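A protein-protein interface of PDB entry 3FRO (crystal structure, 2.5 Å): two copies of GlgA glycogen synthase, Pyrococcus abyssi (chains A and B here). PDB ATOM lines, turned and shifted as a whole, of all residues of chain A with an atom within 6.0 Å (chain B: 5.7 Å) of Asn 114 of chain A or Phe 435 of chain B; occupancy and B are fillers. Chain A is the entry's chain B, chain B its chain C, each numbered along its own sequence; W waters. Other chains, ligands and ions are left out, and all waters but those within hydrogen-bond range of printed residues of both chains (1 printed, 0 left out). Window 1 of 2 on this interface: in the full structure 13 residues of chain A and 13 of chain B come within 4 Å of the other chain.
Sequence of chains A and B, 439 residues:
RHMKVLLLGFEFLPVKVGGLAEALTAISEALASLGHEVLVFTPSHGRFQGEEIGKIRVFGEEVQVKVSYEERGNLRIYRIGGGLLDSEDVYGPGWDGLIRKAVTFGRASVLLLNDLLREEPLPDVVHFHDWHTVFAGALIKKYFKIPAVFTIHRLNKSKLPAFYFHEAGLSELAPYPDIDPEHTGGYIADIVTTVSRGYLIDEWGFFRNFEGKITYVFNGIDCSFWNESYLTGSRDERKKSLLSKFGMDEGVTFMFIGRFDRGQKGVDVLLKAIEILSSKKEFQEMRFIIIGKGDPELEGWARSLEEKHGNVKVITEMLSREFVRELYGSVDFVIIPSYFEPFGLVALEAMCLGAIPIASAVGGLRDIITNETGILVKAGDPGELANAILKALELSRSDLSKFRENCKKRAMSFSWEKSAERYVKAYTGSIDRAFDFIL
Water W1 lies within hydrogen-bond range of O of Phe 144 of chain A (2.7 Å) and NH2 of Arg 433 of chain B (2.9 Å).
Of the 12 printed residues of chain A, 6 touch a printed residue of chain B. Hydrophobic or aromatic side chains of chain A within 4 Å of the printed part of chain B: Val 110, Leu 117, Tyr 143 and Phe 144.
The backbone carbonyl oxygen (O) of Ile 431 of chain B sits at hydrogen-bond distance from the guanidinium group (NH1) of Arg 433 of chain B, at 3.2 Å. O of Gly 212 of chain B is in hydrogen-bond range of NE of Arg 433 of chain B, at 2.8 Å. N of Asp 436 of chain B sits at hydrogen-bond distance from OE2 of Glu 211 of chain B, 2.9 Å away. The backbone carbonyl oxygen (O) of Ala 434 of chain B is in hydrogen-bond range of the backbone NH (N) of Gly 212 of chain B, 3.2 Å away. The guanidinium group (NH2) of Arg 118 of chain A is in salt-bridge range of the side-chain carboxylate (OD1) of Asp 115 of chain A.
Leu 111 of chain A touches none of the printed residues of chain B. Of chain B, only Asp 432, Arg 433, Phe 435 and Ile 438 come within 4 Å of Asn 114 of chain A. Of the printed residues of chain B, Arg 118 of chain A touches Asp 432. Of the printed residues of chain A, Gly 212 of chain B touches Tyr 143 (3.7 Å). The nearest printed residue of chain A that does not touch Phe 435 of chain B is Leu 111 of chain A (6.5 Å). The nearest printed residue of chain B that does not touch Val 110 of chain A is Ile 438 of chain B (5.5 Å).
O of Tyr 143 of chain A sits at hydrogen-bond distance from NH2 of Arg 433 of chain B (3.3 Å). The side-chain amide nitrogen (ND2) of Asn 114 of chain A lies within hydrogen-bond range of the backbone carbonyl oxygen (O) of Arg 433 of chain B (2.8 Å).
No position is printed for both chains. Of the 14 pairs that touch across the chains among the printed residues, none has its exchanged pair printed and touching as well.
Phe 435 of chain B touches Val 110 of chain A (CZ to CG1, 3.8 Å). CG1 of Val 110 of chain A touches CZ of Phe 437 of chain B, 3.8 Å away. Phe 435 of chain B touches Asn 114 of chain A. Asn 114 of chain A touches Ile 438 of chain B (ND2 to CD1, 3.9 Å). Leu 117 of chain A touches Ile 431 of chain B (O to CA, 3.6 Å). CG of Arg 118 of chain A touches OD1 of Asp 432 of chain B, 3.8 Å away. CE2 of Tyr 143 of chain A touches O of Glu 211 of chain B, at 3.3 Å. Phe 435 of chain B touches Tyr 143 of chain A. Phe 144 of chain A touches Arg 433 of chain B (CE2 to NE, 3.5 Å). Phe 435 of chain B touches Phe 144 of chain A.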
ATOM      1  N   SER A 109     -26.756  27.725  27.946  1.00  0.00           N
ATOM      2  CA  SER A 109     -25.490  27.166  27.459  1.00  0.00           C
ATOM      3  C   SER A 109     -25.444  25.650  27.616  1.00  0.00           C
ATOM      4  O   SER A 109     -24.937  24.950  26.739  1.00  0.00           O
ATOM      5  CB  SER A 109     -24.297  27.809  28.165  1.00  0.00           C
ATOM      6  OG  SER A 109     -24.124  29.148  27.732  1.00  0.00           O
ATOM      7  N   VAL A 110     -25.983  25.150  28.727  1.00  0.00           N
ATOM      8  CA  VAL A 110     -26.085  23.705  28.955  1.00  0.00           C
ATOM      9  C   VAL A 110     -26.995  23.064  27.912  1.00  0.00           C
ATOM     10  O   VAL A 110     -26.666  22.011  27.369  1.00  0.00           O
ATOM     11  CB  VAL A 110     -26.610  23.377  30.374  1.00  0.00           C
ATOM     12  CG1 VAL A 110     -26.964  21.901  30.490  1.00  0.00           C
ATOM     13  CG2 VAL A 110     -25.576  23.762  31.428  1.00  0.00           C
ATOM     14  N   LEU A 111     -28.128  23.711  27.630  1.00  0.00           N
ATOM     15  CA  LEU A 111     -29.084  23.214  26.639  1.00  0.00           C
ATOM     16  C   LEU A 111     -28.456  23.091  25.255  1.00  0.00           C
ATOM     17  O   LEU A 111     -28.648  22.083  24.577  1.00  0.00           O
ATOM     18  CB  LEU A 111     -30.321  24.118  26.567  1.00  0.00           C
ATOM     19  CG  LEU A 111     -31.312  23.824  25.432  1.00  0.00           C
ATOM     20  CD1 LEU A 111     -31.744  22.358  25.447  1.00  0.00           C
ATOM     21  CD2 LEU A 111     -32.522  24.747  25.502  1.00  0.00           C
ATOM     22  N   LEU A 112     -27.718  24.119  24.841  1.00  0.00           N
ATOM     23  CA  LEU A 112     -27.061  24.118  23.532  1.00  0.00           C
ATOM     24  C   LEU A 112     -25.995  23.020  23.434  1.00  0.00           C
ATOM     25  O   LEU A 112     -25.969  22.268  22.459  1.00  0.00           O
ATOM     26  CB  LEU A 112     -26.439  25.488  23.239  1.00  0.00           C
ATOM     27  CG  LEU A 112     -25.642  25.638  21.937  1.00  0.00           C
ATOM     28  CD1 LEU A 112     -26.459  25.190  20.727  1.00  0.00           C
ATOM     29  CD2 LEU A 112     -25.172  27.078  21.778  1.00  0.00           C
ATOM     30  N   LEU A 113     -25.127  22.934  24.443  1.00  0.00           N
ATOM     31  CA  LEU A 113     -24.081  21.909  24.488  1.00  0.00           C
ATOM     32  C   LEU A 113     -24.698  20.515  24.441  1.00  0.00           C
ATOM     33  O   LEU A 113     -24.277  19.667  23.656  1.00  0.00           O
ATOM     34  CB  LEU A 113     -23.231  22.066  25.756  1.00  0.00           C
ATOM     35  CG  LEU A 113     -22.028  21.130  25.962  1.00  0.00           C
ATOM     36  CD1 LEU A 113     -20.998  21.283  24.853  1.00  0.00           C
ATOM     37  CD2 LEU A 113     -21.384  21.391  27.322  1.00  0.00           C
ATOM     38  N   ASN A 114     -25.706  20.295  25.279  1.00  0.00           N
ATOM     39  CA  ASN A 114     -26.426  19.023  25.311  1.00  0.00           C
ATOM     40  C   ASN A 114     -26.899  18.626  23.907  1.00  0.00           C
ATOM     41  O   ASN A 114     -26.769  17.467  23.513  1.00  0.00           O
ATOM     42  CB  ASN A 114     -27.621  19.112  26.276  1.00  0.00           C
ATOM     43  CG  ASN A 114     -27.957  17.784  26.936  1.00  0.00           C
ATOM     44  OD1 ASN A 114     -27.075  17.003  27.287  1.00  0.00           O
ATOM     45  ND2 ASN A 114     -29.244  17.541  27.141  1.00  0.00           N
ATOM     46  N   ASP A 115     -27.423  19.599  23.160  1.00  0.00           N
ATOM     47  CA  ASP A 115     -27.899  19.376  21.786  1.00  0.00           C
ATOM     48  C   ASP A 115     -26.770  19.111  20.792  1.00  0.00           C
ATOM     49  O   ASP A 115     -26.913  18.265  19.910  1.00  0.00           O
ATOM     50  CB  ASP A 115     -28.733  20.568  21.298  1.00  0.00           C
ATOM     51  CG  ASP A 115     -30.112  20.627  21.941  1.00  0.00           C
ATOM     52  OD1 ASP A 115     -30.409  19.784  22.820  1.00  0.00           O
ATOM     53  OD2 ASP A 115     -30.904  21.519  21.560  1.00  0.00           O
ATOM     54  N   LEU A 116     -25.663  19.836  20.920  1.00  0.00           N
ATOM     55  CA  LEU A 116     -24.487  19.593  20.079  1.00  0.00           C
ATOM     56  C   LEU A 116     -23.911  18.197  20.313  1.00  0.00           C
ATOM     57  O   LEU A 116     -23.518  17.515  19.369  1.00  0.00           O
ATOM     58  CB  LEU A 116     -23.402  20.635  20.348  1.00  0.00           C
ATOM     59  CG  LEU A 116     -23.695  22.072  19.922  1.00  0.00           C
ATOM     60  CD1 LEU A 116     -22.548  22.977  20.360  1.00  0.00           C
ATOM     61  CD2 LEU A 116     -23.922  22.158  18.424  1.00  0.00           C
ATOM     62  N   LEU A 117     -23.876  17.774  21.576  1.00  0.00           N
ATOM     63  CA  LEU A 117     -23.345  16.460  21.948  1.00  0.00           C
ATOM     64  C   LEU A 117     -24.172  15.297  21.405  1.00  0.00           C
ATOM     65  O   LEU A 117     -23.733  14.145  21.446  1.00  0.00           O
ATOM     66  CB  LEU A 117     -23.230  16.340  23.473  1.00  0.00           C
ATOM     67  CG  LEU A 117     -22.127  17.184  24.105  1.00  0.00           C
ATOM     68  CD1 LEU A 117     -22.261  17.190  25.619  1.00  0.00           C
ATOM     69  CD2 LEU A 117     -20.769  16.669  23.678  1.00  0.00           C
ATOM     70  N   ARG A 118     -25.365  15.605  20.907  1.00  0.00           N
ATOM     71  CA  ARG A 118     -26.213  14.620  20.247  1.00  0.00           C
ATOM     72  C   ARG A 118     -25.636  14.180  18.902  1.00  0.00           C
ATOM     73  O   ARG A 118     -25.975  13.102  18.408  1.00  0.00           O
ATOM     74  CB  ARG A 118     -27.614  15.198  20.050  1.00  0.00           C
ATOM     75  CG  ARG A 118     -28.714  14.166  19.850  1.00  0.00           C
ATOM     76  CD  ARG A 118     -30.011  14.660  20.478  1.00  0.00           C
ATOM     77  NE  ARG A 118     -30.360  16.006  20.017  1.00  0.00           N
ATOM     78  CZ  ARG A 118     -31.050  16.909  20.715  1.00  0.00           C
ATOM     79  NH1 ARG A 118     -31.484  16.647  21.949  1.00  0.00           N
ATOM     80  NH2 ARG A 118     -31.302  18.100  20.172  1.00  0.00           N
ATOM     81  N   TYR A 143     -21.522  19.023  35.566  1.00  0.00           N
ATOM     82  CA  TYR A 143     -22.196  17.890  34.935  1.00  0.00           C
ATOM     83  C   TYR A 143     -21.345  17.170  33.900  1.00  0.00           C
ATOM     84  O   TYR A 143     -21.279  15.940  33.902  1.00  0.00           O
ATOM     85  CB  TYR A 143     -23.493  18.358  34.280  1.00  0.00           C
ATOM     86  CG  TYR A 143     -24.531  18.822  35.273  1.00  0.00           C
ATOM     87  CD1 TYR A 143     -24.915  20.156  35.337  1.00  0.00           C
ATOM     88  CD2 TYR A 143     -25.127  17.922  36.154  1.00  0.00           C
ATOM     89  CE1 TYR A 143     -25.872  20.582  36.243  1.00  0.00           C
ATOM     90  CE2 TYR A 143     -26.084  18.339  37.065  1.00  0.00           C
ATOM     91  CZ  TYR A 143     -26.451  19.670  37.104  1.00  0.00           C
ATOM     92  OH  TYR A 143     -27.395  20.094  38.005  1.00  0.00           O
ATOM     93  N   PHE A 144     -20.706  17.927  33.015  1.00  0.00           N
ATOM     94  CA  PHE A 144     -19.945  17.333  31.912  1.00  0.00           C
ATOM     95  C   PHE A 144     -18.517  16.974  32.296  1.00  0.00           C
ATOM     96  O   PHE A 144     -17.857  16.227  31.573  1.00  0.00           O
ATOM     97  CB  PHE A 144     -19.968  18.247  30.686  1.00  0.00           C
ATOM     98  CG  PHE A 144     -21.345  18.488  30.154  1.00  0.00           C
ATOM     99  CD1 PHE A 144     -22.066  19.609  30.542  1.00  0.00           C
ATOM    100  CD2 PHE A 144     -21.936  17.575  29.292  1.00  0.00           C
ATOM    101  CE1 PHE A 144     -23.345  19.831  30.062  1.00  0.00           C
ATOM    102  CE2 PHE A 144     -23.216  17.786  28.807  1.00  0.00           C
ATOM    103  CZ  PHE A 144     -23.924  18.918  29.192  1.00  0.00           C
ATOM    104  N   TRP B 204     -38.545   8.938  36.730  1.00  0.00           N
ATOM    105  CA  TRP B 204     -37.696  10.096  36.998  1.00  0.00           C
ATOM    106  C   TRP B 204     -37.458  10.278  38.496  1.00  0.00           C
ATOM    107  O   TRP B 204     -36.372  10.683  38.899  1.00  0.00           O
ATOM    108  CB  TRP B 204     -38.286  11.373  36.387  1.00  0.00           C
ATOM    109  CG  TRP B 204     -37.369  12.564  36.504  1.00  0.00           C
ATOM    110  CD1 TRP B 204     -37.627  13.736  37.155  1.00  0.00           C
ATOM    111  CD2 TRP B 204     -36.042  12.684  35.974  1.00  0.00           C
ATOM    112  NE1 TRP B 204     -36.550  14.583  37.052  1.00  0.00           N
ATOM    113  CE2 TRP B 204     -35.563  13.961  36.334  1.00  0.00           C
ATOM    114  CE3 TRP B 204     -35.214  11.839  35.223  1.00  0.00           C
ATOM    115  CZ2 TRP B 204     -34.294  14.417  35.968  1.00  0.00           C
ATOM    116  CZ3 TRP B 204     -33.951  12.292  34.860  1.00  0.00           C
ATOM    117  CH2 TRP B 204     -33.505  13.569  35.234  1.00  0.00           C
ATOM    118  N   GLU B 211     -29.118  13.314  37.565  1.00  0.00           N
ATOM    119  CA  GLU B 211     -29.379  14.424  36.656  1.00  0.00           C
ATOM    120  C   GLU B 211     -28.081  14.946  36.048  1.00  0.00           C
ATOM    121  O   GLU B 211     -27.138  15.264  36.772  1.00  0.00           O
ATOM    122  CB  GLU B 211     -30.086  15.548  37.419  1.00  0.00           C
ATOM    123  CG  GLU B 211     -30.405  16.788  36.594  1.00  0.00           C
ATOM    124  CD  GLU B 211     -31.181  17.828  37.381  1.00  0.00           C
ATOM    125  OE1 GLU B 211     -31.123  17.806  38.633  1.00  0.00           O
ATOM    126  OE2 GLU B 211     -31.847  18.673  36.748  1.00  0.00           O
ATOM    127  N   GLY B 212     -28.040  15.018  34.718  1.00  0.00           N
ATOM    128  CA  GLY B 212     -26.866  15.513  33.997  1.00  0.00           C
ATOM    129  C   GLY B 212     -25.832  14.460  33.627  1.00  0.00           C
ATOM    130  O   GLY B 212     -24.867  14.767  32.925  1.00  0.00           O
ATOM    131  N   ILE B 431     -22.261  12.635  24.685  1.00  0.00           N
ATOM    132  CA  ILE B 431     -23.663  12.277  24.550  1.00  0.00           C
ATOM    133  C   ILE B 431     -24.520  13.263  25.337  1.00  0.00           C
ATOM    134  O   ILE B 431     -24.052  13.868  26.298  1.00  0.00           O
ATOM    135  CB  ILE B 431     -23.899  10.832  25.049  1.00  0.00           C
ATOM    136  CG1 ILE B 431     -25.288  10.334  24.651  1.00  0.00           C
ATOM    137  CG2 ILE B 431     -23.699  10.740  26.560  1.00  0.00           C
ATOM    138  CD1 ILE B 431     -25.424   8.833  24.718  1.00  0.00           C
ATOM    139  N   ASP B 432     -25.767  13.438  24.912  1.00  0.00           N
ATOM    140  CA  ASP B 432     -26.718  14.279  25.641  1.00  0.00           C
ATOM    141  C   ASP B 432     -27.271  13.532  26.851  1.00  0.00           C
ATOM    142  O   ASP B 432     -27.170  12.307  26.935  1.00  0.00           O
ATOM    143  CB  ASP B 432     -27.869  14.715  24.734  1.00  0.00           C
ATOM    144  CG  ASP B 432     -28.637  13.542  24.162  1.00  0.00           C
ATOM    145  OD1 ASP B 432     -28.046  12.788  23.362  1.00  0.00           O
ATOM    146  OD2 ASP B 432     -29.826  13.379  24.509  1.00  0.00           O
ATOM    147  N   ARG B 433     -27.869  14.275  27.777  1.00  0.00           N
ATOM    148  CA  ARG B 433     -28.376  13.704  29.028  1.00  0.00           C
ATOM    149  C   ARG B 433     -29.598  14.469  29.533  1.00  0.00           C
ATOM    150  O   ARG B 433     -29.916  15.552  29.033  1.00  0.00           O
ATOM    151  CB  ARG B 433     -27.273  13.675  30.096  1.00  0.00           C
ATOM    152  CG  ARG B 433     -26.293  14.844  30.011  1.00  0.00           C
ATOM    153  CD  ARG B 433     -24.971  14.466  29.343  1.00  0.00           C
ATOM    154  NE  ARG B 433     -23.860  14.626  30.271  1.00  0.00           N
ATOM    155  CZ  ARG B 433     -22.624  14.185  30.061  1.00  0.00           C
ATOM    156  NH1 ARG B 433     -22.296  13.554  28.944  1.00  0.00           N
ATOM    157  NH2 ARG B 433     -21.701  14.386  30.985  1.00  0.00           N
ATOM    158  N   ALA B 434     -30.278  13.896  30.523  1.00  0.00           N
ATOM    159  CA  ALA B 434     -31.551  14.429  31.010  1.00  0.00           C
ATOM    160  C   ALA B 434     -31.351  15.478  32.101  1.00  0.00           C
ATOM    161  O   ALA B 434     -30.767  15.185  33.147  1.00  0.00           O
ATOM    162  CB  ALA B 434     -32.427  13.297  31.525  1.00  0.00           C
ATOM    163  N   PHE B 435     -31.834  16.694  31.846  1.00  0.00           N
ATOM    164  CA  PHE B 435     -31.827  17.777  32.828  1.00  0.00           C
ATOM    165  C   PHE B 435     -33.253  18.218  33.150  1.00  0.00           C
ATOM    166  O   PHE B 435     -34.049  18.485  32.253  1.00  0.00           O
ATOM    167  CB  PHE B 435     -31.069  18.988  32.299  1.00  0.00           C
ATOM    168  CG  PHE B 435     -29.610  18.750  32.083  1.00  0.00           C
ATOM    169  CD1 PHE B 435     -28.690  19.095  33.057  1.00  0.00           C
ATOM    170  CD2 PHE B 435     -29.154  18.205  30.894  1.00  0.00           C
ATOM    171  CE1 PHE B 435     -27.340  18.890  32.855  1.00  0.00           C
ATOM    172  CE2 PHE B 435     -27.812  18.000  30.682  1.00  0.00           C
ATOM    173  CZ  PHE B 435     -26.898  18.340  31.666  1.00  0.00           C
ATOM    174  N   ASP B 436     -33.549  18.332  34.439  1.00  0.00           N
ATOM    175  CA  ASP B 436     -34.882  18.688  34.910  1.00  0.00           C
ATOM    176  C   ASP B 436     -35.382  20.022  34.348  1.00  0.00           C
ATOM    177  O   ASP B 436     -36.573  20.179  34.086  1.00  0.00           O
ATOM    178  CB  ASP B 436     -34.882  18.743  36.442  1.00  0.00           C
ATOM    179  CG  ASP B 436     -36.275  18.774  37.023  1.00  0.00           C
ATOM    180  OD1 ASP B 436     -37.073  17.868  36.698  1.00  0.00           O
ATOM    181  OD2 ASP B 436     -36.569  19.701  37.808  1.00  0.00           O
ATOM    182  N   PHE B 437     -34.467  20.969  34.153  1.00  0.00           N
ATOM    183  CA  PHE B 437     -34.827  22.331  33.739  1.00  0.00           C
ATOM    184  C   PHE B 437     -35.021  22.513  32.225  1.00  0.00           C
ATOM    185  O   PHE B 437     -35.307  23.619  31.776  1.00  0.00           O
ATOM    186  CB  PHE B 437     -33.805  23.351  34.275  1.00  0.00           C
ATOM    187  CG  PHE B 437     -32.408  23.163  33.745  1.00  0.00           C
ATOM    188  CD1 PHE B 437     -32.044  23.674  32.506  1.00  0.00           C
ATOM    189  CD2 PHE B 437     -31.455  22.483  34.489  1.00  0.00           C
ATOM    190  CE1 PHE B 437     -30.756  23.502  32.016  1.00  0.00           C
ATOM    191  CE2 PHE B 437     -30.167  22.307  34.004  1.00  0.00           C
ATOM    192  CZ  PHE B 437     -29.817  22.819  32.767  1.00  0.00           C
ATOM    193  N   ILE B 438     -34.866  21.445  31.445  1.00  0.00           N
ATOM    194  CA  ILE B 438     -35.156  21.490  30.009  1.00  0.00           C
ATOM    195  C   ILE B 438     -36.628  21.150  29.769  1.00  0.00           C
ATOM    196  O   ILE B 438     -37.108  20.112  30.224  1.00  0.00           O
ATOM    197  CB  ILE B 438     -34.257  20.523  29.210  1.00  0.00           C
ATOM    198  CG1 ILE B 438     -32.820  21.054  29.163  1.00  0.00           C
ATOM    199  CG2 ILE B 438     -34.784  20.344  27.792  1.00  0.00           C
ATOM    200  CD1 ILE B 438     -31.795  20.020  28.728  1.00  0.00           C
HETATM  201  O   HOH W   1     -19.001  13.850  31.870  1.00  0.00           O
